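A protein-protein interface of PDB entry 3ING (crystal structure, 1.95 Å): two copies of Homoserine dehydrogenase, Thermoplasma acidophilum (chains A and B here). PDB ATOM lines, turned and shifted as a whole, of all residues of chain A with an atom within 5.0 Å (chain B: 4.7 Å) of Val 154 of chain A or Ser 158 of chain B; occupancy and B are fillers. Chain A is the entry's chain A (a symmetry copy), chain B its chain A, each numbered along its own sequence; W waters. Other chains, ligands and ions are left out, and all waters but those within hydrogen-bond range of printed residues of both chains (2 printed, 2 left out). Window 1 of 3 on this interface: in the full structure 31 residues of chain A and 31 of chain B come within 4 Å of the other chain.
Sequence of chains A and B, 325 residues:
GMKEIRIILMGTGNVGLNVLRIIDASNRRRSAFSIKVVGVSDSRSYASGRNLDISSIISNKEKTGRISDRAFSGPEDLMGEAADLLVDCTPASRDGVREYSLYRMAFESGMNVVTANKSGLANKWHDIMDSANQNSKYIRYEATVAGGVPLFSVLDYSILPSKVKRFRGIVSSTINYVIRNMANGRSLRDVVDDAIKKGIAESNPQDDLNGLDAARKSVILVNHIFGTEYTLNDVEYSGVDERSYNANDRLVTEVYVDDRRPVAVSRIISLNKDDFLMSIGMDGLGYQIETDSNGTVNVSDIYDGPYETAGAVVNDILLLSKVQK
OG of Ser 153 of chain B lies within hydrogen-bond range of OG of Ser 158 of chain A, at 2.7 Å. O of Tyr 157 of chain B sits close to OD1 of Asn 315 of chain A. The side-chain hydroxyl of Ser 153 of chain A lies within hydrogen-bond range of the side-chain hydroxyl of Ser 158 of chain B (2.7 Å). O of Ser 158 of chain B sits close to ND2 of Asn 315 of chain A (3.4 Å). N of Ile 159 of chain B lies close to ND2 of Asn 315 of chain A (3.5 Å). The side-chain amide nitrogen of Asn 315 of chain A lies close to the backbone NH of Leu 160 of chain B.
The backbone carbonyl oxygen (O) of Val 154 of chain B lies within hydrogen-bond range of the backbone NH (N) of Ile 159 of chain B (3.4 Å). The backbone carbonyl oxygen of Pro 150 of chain A is in hydrogen-bond range of the side-chain hydroxyl of Tyr 287 of chain A. The backbone carbonyl oxygen (O) of Val 154 of chain A sits at hydrogen-bond distance from the backbone NH (N) of Ile 159 of chain A, at 3.4 Å.
Among the printed residues, merely in contact across the chains: Pro 150 of chain A with Ser 158 of chain B (3.8 Å), Ser 153 of chain A with Tyr 157 of chain B (3.7 Å), Val 154 of chain A with Ser 158 of chain B (3.9 Å), Tyr 157 of chain A with Ser 153 of chain B (3.7 Å), Tyr 157 of chain A with Tyr 157 of chain B (3.9 Å) and Ser 158 of chain A with Val 154 of chain B (3.9 Å).
Of chain B, only Ser 158 (3.9 Å) comes within 4 Å of Val 154 of chain A. Of chain A, only Pro 150 (3.8 Å), Ser 153 (2.7 Å), Val 154 (3.9 Å) and Asn 315 (3.3 Å) come within 4 Å of Ser 158 of chain B. Of the printed residues of chain A, Tyr 157 of chain B touches Ser 153, Tyr 157 and Asn 315. Printed residues of chain B within 4 Å of Ser 158 of chain A: Ser 153 (2.7 Å) and Val 154 (3.9 Å). Asp 156 of chain A touches none of the printed residues of chain B. Asn 294 of chain B touches none of the printed residues of chain A. The nearest printed residue of chain A that does not touch Ser 158 of chain B is Ser 158 of chain A (5.1 Å). The nearest printed residue of chain B that does not touch Ser 158 of chain A is Ser 158 of chain B (5.1 Å).
Of the 8 printed residues of chain B, 6 touch a printed residue of chain A. Printed residues of chain B that touch a printed residue of chain A: Ser 153, Val 154, Tyr 157, Ser 158, Ile 159 and Leu 160. Hydrophobic or aromatic side chains of chain B that line the printed part of chain A: Val 154, Tyr 157 and Leu 160. Of the 14 printed residues of chain A, 6 touch a printed residue of chain B.
Ser 153 of chain A touches Tyr 157 of chain B, and with the chains exchanged Tyr 157 of chain A touches Ser 153 of chain B. Ser 153 of chain A touches Ser 158 of chain B, and with the chains exchanged Ser 158 of chain A touches Ser 153 of chain B. Val 154 of chain A touches Ser 158 of chain B, and with the chains exchanged Ser 158 of chain A touches Val 154 of chain B. Tyr 157 of chain B touches its own counterpart, Tyr 157 of chain A. Of the 12 pairs that touch across the chains among the printed residues, 7 have their exchanged pair printed and touching as well.
Water W2 bridges OG of Ser 153 of chain B (2.7 Å) and O of Ser 158 of chain A (3.0 Å). Water W1 lies within hydrogen-bond range of OG of Ser 153 of chain A and O of Ser 158 of chain B.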
ATOM      1  N   PRO A 150     -29.002  -2.645 -33.979  1.00  0.00           N
ATOM      2  CA  PRO A 150     -28.554  -3.775 -33.160  1.00  0.00           C
ATOM      3  C   PRO A 150     -29.646  -4.814 -32.950  1.00  0.00           C
ATOM      4  O   PRO A 150     -30.751  -4.502 -32.493  1.00  0.00           O
ATOM      5  CB  PRO A 150     -28.175  -3.124 -31.822  1.00  0.00           C
ATOM      6  CG  PRO A 150     -27.918  -1.693 -32.165  1.00  0.00           C
ATOM      7  CD  PRO A 150     -28.872  -1.363 -33.275  1.00  0.00           C
ATOM      8  N   LEU A 151     -29.326  -6.066 -33.282  1.00  0.00           N
ATOM      9  CA  LEU A 151     -30.289  -7.126 -33.276  1.00  0.00           C
ATOM     10  C   LEU A 151     -29.618  -8.362 -32.683  1.00  0.00           C
ATOM     11  O   LEU A 151     -29.964  -8.785 -31.574  1.00  0.00           O
ATOM     12  CB  LEU A 151     -30.797  -7.348 -34.727  1.00  0.00           C
ATOM     13  CG  LEU A 151     -32.110  -8.116 -34.903  1.00  0.00           C
ATOM     14  CD1 LEU A 151     -32.712  -7.946 -36.318  1.00  0.00           C
ATOM     15  CD2 LEU A 151     -31.955  -9.559 -34.565  1.00  0.00           C
ATOM     16  N   PHE A 152     -28.647  -8.946 -33.379  1.00  0.00           N
ATOM     17  CA  PHE A 152     -28.073 -10.203 -32.850  1.00  0.00           C
ATOM     18  C   PHE A 152     -27.256  -9.947 -31.602  1.00  0.00           C
ATOM     19  O   PHE A 152     -27.228 -10.788 -30.695  1.00  0.00           O
ATOM     20  CB  PHE A 152     -27.345 -10.996 -33.939  1.00  0.00           C
ATOM     21  CG  PHE A 152     -28.269 -11.484 -35.002  1.00  0.00           C
ATOM     22  CD1 PHE A 152     -29.266 -12.411 -34.708  1.00  0.00           C
ATOM     23  CD2 PHE A 152     -28.245 -10.939 -36.244  1.00  0.00           C
ATOM     24  CE1 PHE A 152     -30.150 -12.803 -35.656  1.00  0.00           C
ATOM     25  CE2 PHE A 152     -29.118 -11.367 -37.213  1.00  0.00           C
ATOM     26  CZ  PHE A 152     -30.073 -12.299 -36.913  1.00  0.00           C
ATOM     27  N   SER A 153     -26.627  -8.794 -31.518  1.00  0.00           N
ATOM     28  CA  SER A 153     -25.850  -8.440 -30.320  1.00  0.00           C
ATOM     29  C   SER A 153     -26.804  -8.273 -29.112  1.00  0.00           C
ATOM     30  O   SER A 153     -26.440  -8.557 -27.954  1.00  0.00           O
ATOM     31  CB  SER A 153     -25.054  -7.171 -30.581  1.00  0.00           C
ATOM     32  OG  SER A 153     -25.821  -6.034 -30.995  1.00  0.00           O
ATOM     33  N   VAL A 154     -28.024  -7.796 -29.403  1.00  0.00           N
ATOM     34  CA  VAL A 154     -29.087  -7.642 -28.371  1.00  0.00           C
ATOM     35  C   VAL A 154     -29.560  -9.018 -27.903  1.00  0.00           C
ATOM     36  O   VAL A 154     -29.710  -9.302 -26.698  1.00  0.00           O
ATOM     37  CB  VAL A 154     -30.246  -6.830 -28.928  1.00  0.00           C
ATOM     38  CG1 VAL A 154     -31.471  -6.833 -27.983  1.00  0.00           C
ATOM     39  CG2 VAL A 154     -29.762  -5.389 -29.258  1.00  0.00           C
ATOM     40  N   LEU A 155     -29.812  -9.875 -28.878  1.00  0.00           N
ATOM     41  CA  LEU A 155     -30.265 -11.242 -28.590  1.00  0.00           C
ATOM     42  C   LEU A 155     -29.171 -12.008 -27.872  1.00  0.00           C
ATOM     43  O   LEU A 155     -29.476 -12.786 -26.965  1.00  0.00           O
ATOM     44  CB  LEU A 155     -30.693 -11.965 -29.870  1.00  0.00           C
ATOM     45  CG  LEU A 155     -31.939 -11.494 -30.623  1.00  0.00           C
ATOM     46  CD1 LEU A 155     -32.087 -12.240 -31.889  1.00  0.00           C
ATOM     47  CD2 LEU A 155     -33.173 -11.661 -29.785  1.00  0.00           C
ATOM     48  N   ASP A 156     -27.898 -11.771 -28.218  1.00  0.00           N
ATOM     49  CA  ASP A 156     -26.784 -12.482 -27.571  1.00  0.00           C
ATOM     50  C   ASP A 156     -26.424 -11.965 -26.171  1.00  0.00           C
ATOM     51  O   ASP A 156     -26.007 -12.724 -25.328  1.00  0.00           O
ATOM     52  CB  ASP A 156     -25.491 -12.395 -28.410  1.00  0.00           C
ATOM     53  CG  ASP A 156     -25.524 -13.255 -29.672  1.00  0.00           C
ATOM     54  OD1 ASP A 156     -26.392 -14.127 -29.748  1.00  0.00           O
ATOM     55  OD2 ASP A 156     -24.670 -13.052 -30.575  1.00  0.00           O
ATOM     56  N   TYR A 157     -26.498 -10.661 -25.940  1.00  0.00           N
ATOM     57  CA  TYR A 157     -25.965 -10.121 -24.688  1.00  0.00           C
ATOM     58  C   TYR A 157     -26.888  -9.284 -23.820  1.00  0.00           C
ATOM     59  O   TYR A 157     -26.465  -8.866 -22.737  1.00  0.00           O
ATOM     60  CB  TYR A 157     -24.721  -9.266 -25.016  1.00  0.00           C
ATOM     61  CG  TYR A 157     -23.686 -10.035 -25.784  1.00  0.00           C
ATOM     62  CD1 TYR A 157     -22.945 -11.041 -25.163  1.00  0.00           C
ATOM     63  CD2 TYR A 157     -23.487  -9.822 -27.137  1.00  0.00           C
ATOM     64  CE1 TYR A 157     -22.037 -11.775 -25.870  1.00  0.00           C
ATOM     65  CE2 TYR A 157     -22.586 -10.561 -27.842  1.00  0.00           C
ATOM     66  CZ  TYR A 157     -21.842 -11.514 -27.199  1.00  0.00           C
ATOM     67  OH  TYR A 157     -20.907 -12.273 -27.891  1.00  0.00           O
ATOM     68  N   SER A 158     -28.107  -9.006 -24.285  1.00  0.00           N
ATOM     69  CA  SER A 158     -29.040  -8.154 -23.542  1.00  0.00           C
ATOM     70  C   SER A 158     -30.244  -8.887 -22.951  1.00  0.00           C
ATOM     71  O   SER A 158     -30.838  -8.392 -22.004  1.00  0.00           O
ATOM     72  CB  SER A 158     -29.561  -7.029 -24.430  1.00  0.00           C
ATOM     73  OG  SER A 158     -28.554  -6.071 -24.745  1.00  0.00           O
ATOM     74  N   ILE A 159     -30.608 -10.048 -23.486  1.00  0.00           N
ATOM     75  CA  ILE A 159     -31.768 -10.817 -22.976  1.00  0.00           C
ATOM     76  C   ILE A 159     -31.442 -12.298 -22.737  1.00  0.00           C
ATOM     77  O   ILE A 159     -32.223 -13.200 -23.022  1.00  0.00           O
ATOM     78  CB  ILE A 159     -32.982 -10.672 -23.919  1.00  0.00           C
ATOM     79  CG1 ILE A 159     -32.644 -11.199 -25.334  1.00  0.00           C
ATOM     80  CG2 ILE A 159     -33.387  -9.258 -24.013  1.00  0.00           C
ATOM     81  CD1 ILE A 159     -33.852 -11.296 -26.256  1.00  0.00           C
ATOM     82  N   TYR A 287     -37.550  -3.331 -35.049  1.00  0.00           N
ATOM     83  CA  TYR A 287     -38.248  -4.530 -34.703  1.00  0.00           C
ATOM     84  C   TYR A 287     -38.726  -4.564 -33.238  1.00  0.00           C
ATOM     85  O   TYR A 287     -38.403  -3.692 -32.398  1.00  0.00           O
ATOM     86  CB  TYR A 287     -37.336  -5.746 -34.958  1.00  0.00           C
ATOM     87  CG  TYR A 287     -36.113  -5.754 -34.047  1.00  0.00           C
ATOM     88  CD1 TYR A 287     -36.174  -6.280 -32.787  1.00  0.00           C
ATOM     89  CD2 TYR A 287     -34.916  -5.201 -34.456  1.00  0.00           C
ATOM     90  CE1 TYR A 287     -35.055  -6.275 -31.920  1.00  0.00           C
ATOM     91  CE2 TYR A 287     -33.812  -5.182 -33.606  1.00  0.00           C
ATOM     92  CZ  TYR A 287     -33.887  -5.731 -32.342  1.00  0.00           C
ATOM     93  OH  TYR A 287     -32.763  -5.730 -31.492  1.00  0.00           O
ATOM     94  N   ILE A 289     -39.125  -7.598 -30.084  1.00  0.00           N
ATOM     95  CA  ILE A 289     -39.015  -8.968 -29.652  1.00  0.00           C
ATOM     96  C   ILE A 289     -39.802  -9.153 -28.373  1.00  0.00           C
ATOM     97  O   ILE A 289     -39.585  -8.475 -27.373  1.00  0.00           O
ATOM     98  CB  ILE A 289     -37.573  -9.462 -29.405  1.00  0.00           C
ATOM     99  CG1 ILE A 289     -36.728  -8.378 -28.754  1.00  0.00           C
ATOM    100  CG2 ILE A 289     -36.963 -10.018 -30.697  1.00  0.00           C
ATOM    101  CD1 ILE A 289     -35.454  -8.907 -28.209  1.00  0.00           C
ATOM    102  N   VAL A 299     -36.655  -1.887 -30.829  1.00  0.00           N
ATOM    103  CA  VAL A 299     -35.335  -1.356 -31.224  1.00  0.00           C
ATOM    104  C   VAL A 299     -35.480  -0.849 -32.638  1.00  0.00           C
ATOM    105  O   VAL A 299     -36.108  -1.512 -33.481  1.00  0.00           O
ATOM    106  CB  VAL A 299     -34.223  -2.407 -31.164  1.00  0.00           C
ATOM    107  CG1 VAL A 299     -32.834  -1.766 -31.484  1.00  0.00           C
ATOM    108  CG2 VAL A 299     -34.196  -3.149 -29.805  1.00  0.00           C
ATOM    109  N   ASN A 315     -18.596  -3.704 -35.122  1.00  0.00           N
ATOM    110  CA  ASN A 315     -18.983  -4.189 -33.788  1.00  0.00           C
ATOM    111  C   ASN A 315     -18.747  -5.693 -33.699  1.00  0.00           C
ATOM    112  O   ASN A 315     -18.181  -6.181 -32.723  1.00  0.00           O
ATOM    113  CB  ASN A 315     -20.436  -3.872 -33.453  1.00  0.00           C
ATOM    114  CG  ASN A 315     -20.745  -4.146 -32.011  1.00  0.00           C
ATOM    115  OD1 ASN A 315     -21.390  -5.161 -31.657  1.00  0.00           O
ATOM    116  ND2 ASN A 315     -20.200  -3.304 -31.150  1.00  0.00           N
ATOM    117  N   SER B 153     -26.059  -2.912 -21.460  1.00  0.00           N
ATOM    118  CA  SER B 153     -25.636  -4.078 -22.250  1.00  0.00           C
ATOM    119  C   SER B 153     -25.518  -3.680 -23.742  1.00  0.00           C
ATOM    120  O   SER B 153     -24.676  -4.211 -24.491  1.00  0.00           O
ATOM    121  CB  SER B 153     -26.623  -5.217 -22.055  1.00  0.00           C
ATOM    122  OG  SER B 153     -27.989  -4.913 -22.363  1.00  0.00           O
ATOM    123  N   VAL B 154     -26.386  -2.745 -24.159  1.00  0.00           N
ATOM    124  CA  VAL B 154     -26.362  -2.196 -25.544  1.00  0.00           C
ATOM    125  C   VAL B 154     -25.106  -1.349 -25.745  1.00  0.00           C
ATOM    126  O   VAL B 154     -24.382  -1.453 -26.756  1.00  0.00           O
ATOM    127  CB  VAL B 154     -27.617  -1.376 -25.804  1.00  0.00           C
ATOM    128  CG1 VAL B 154     -27.540  -0.596 -27.138  1.00  0.00           C
ATOM    129  CG2 VAL B 154     -28.867  -2.299 -25.734  1.00  0.00           C
ATOM    130  N   ASP B 156     -22.420  -1.536 -23.957  1.00  0.00           N
ATOM    131  CA  ASP B 156     -21.227  -2.386 -23.823  1.00  0.00           C
ATOM    132  C   ASP B 156     -20.970  -3.320 -25.013  1.00  0.00           C
ATOM    133  O   ASP B 156     -19.840  -3.607 -25.332  1.00  0.00           O
ATOM    134  CB  ASP B 156     -21.312  -3.290 -22.574  1.00  0.00           C
ATOM    135  CG  ASP B 156     -21.125  -2.533 -21.259  1.00  0.00           C
ATOM    136  OD1 ASP B 156     -20.644  -1.400 -21.314  1.00  0.00           O
ATOM    137  OD2 ASP B 156     -21.456  -3.090 -20.179  1.00  0.00           O
ATOM    138  N   TYR B 157     -22.013  -3.869 -25.622  1.00  0.00           N
ATOM    139  CA  TYR B 157     -21.792  -4.919 -26.619  1.00  0.00           C
ATOM    140  C   TYR B 157     -22.389  -4.728 -28.002  1.00  0.00           C
ATOM    141  O   TYR B 157     -22.167  -5.582 -28.867  1.00  0.00           O
ATOM    142  CB  TYR B 157     -22.331  -6.251 -26.052  1.00  0.00           C
ATOM    143  CG  TYR B 157     -21.718  -6.596 -24.726  1.00  0.00           C
ATOM    144  CD1 TYR B 157     -20.384  -6.994 -24.643  1.00  0.00           C
ATOM    145  CD2 TYR B 157     -22.431  -6.461 -23.546  1.00  0.00           C
ATOM    146  CE1 TYR B 157     -19.810  -7.261 -23.434  1.00  0.00           C
ATOM    147  CE2 TYR B 157     -21.855  -6.722 -22.341  1.00  0.00           C
ATOM    148  CZ  TYR B 157     -20.555  -7.150 -22.291  1.00  0.00           C
ATOM    149  OH  TYR B 157     -19.946  -7.436 -21.076  1.00  0.00           O
ATOM    150  N   SER B 158     -23.161  -3.660 -28.211  1.00  0.00           N
ATOM    151  CA  SER B 158     -23.827  -3.430 -29.497  1.00  0.00           C
ATOM    152  C   SER B 158     -23.269  -2.260 -30.307  1.00  0.00           C
ATOM    153  O   SER B 158     -23.448  -2.232 -31.516  1.00  0.00           O
ATOM    154  CB  SER B 158     -25.319  -3.194 -29.291  1.00  0.00           C
ATOM    155  OG  SER B 158     -26.005  -4.368 -28.868  1.00  0.00           O
ATOM    156  N   ILE B 159     -22.600  -1.305 -29.669  1.00  0.00           N
ATOM    157  CA  ILE B 159     -22.034  -0.134 -30.380  1.00  0.00           C
ATOM    158  C   ILE B 159     -20.569   0.135 -30.012  1.00  0.00           C
ATOM    159  O   ILE B 159     -20.128   1.267 -29.842  1.00  0.00           O
ATOM    160  CB  ILE B 159     -22.896   1.125 -30.140  1.00  0.00           C
ATOM    161  CG1 ILE B 159     -22.961   1.466 -28.633  1.00  0.00           C
ATOM    162  CG2 ILE B 159     -24.263   0.909 -30.648  1.00  0.00           C
ATOM    163  CD1 ILE B 159     -23.604   2.815 -28.338  1.00  0.00           C
ATOM    164  N   LEU B 160     -19.792  -0.936 -29.925  1.00  0.00           N
ATOM    165  CA  LEU B 160     -18.365  -0.845 -29.583  1.00  0.00           C
ATOM    166  C   LEU B 160     -17.528   0.130 -30.433  1.00  0.00           C
ATOM    167  O   LEU B 160     -16.649   0.795 -29.910  1.00  0.00           O
ATOM    168  CB  LEU B 160     -17.715  -2.246 -29.601  1.00  0.00           C
ATOM    169  CG  LEU B 160     -18.075  -3.161 -28.428  1.00  0.00           C
ATOM    170  CD1 LEU B 160     -17.747  -4.582 -28.765  1.00  0.00           C
ATOM    171  CD2 LEU B 160     -17.299  -2.667 -27.149  1.00  0.00           C
ATOM    172  N   ASN B 294     -22.494   4.078 -35.368  1.00  0.00           N
ATOM    173  CA  ASN B 294     -23.625   3.139 -35.393  1.00  0.00           C
ATOM    174  C   ASN B 294     -24.963   3.849 -35.525  1.00  0.00           C
ATOM    175  O   ASN B 294     -26.015   3.276 -35.183  1.00  0.00           O
ATOM    176  CB  ASN B 294     -23.599   2.267 -34.114  1.00  0.00           C
ATOM    177  CG  ASN B 294     -22.387   1.357 -34.066  1.00  0.00           C
ATOM    178  OD1 ASN B 294     -22.419   0.250 -34.646  1.00  0.00           O
ATOM    179  ND2 ASN B 294     -21.290   1.817 -33.412  1.00  0.00           N
HETATM  180  O   HOH W   1     -24.858  -4.438 -32.887  1.00  0.00           O
HETATM  181  O   HOH W   2     -29.915  -5.857 -20.798  1.00  0.00           O
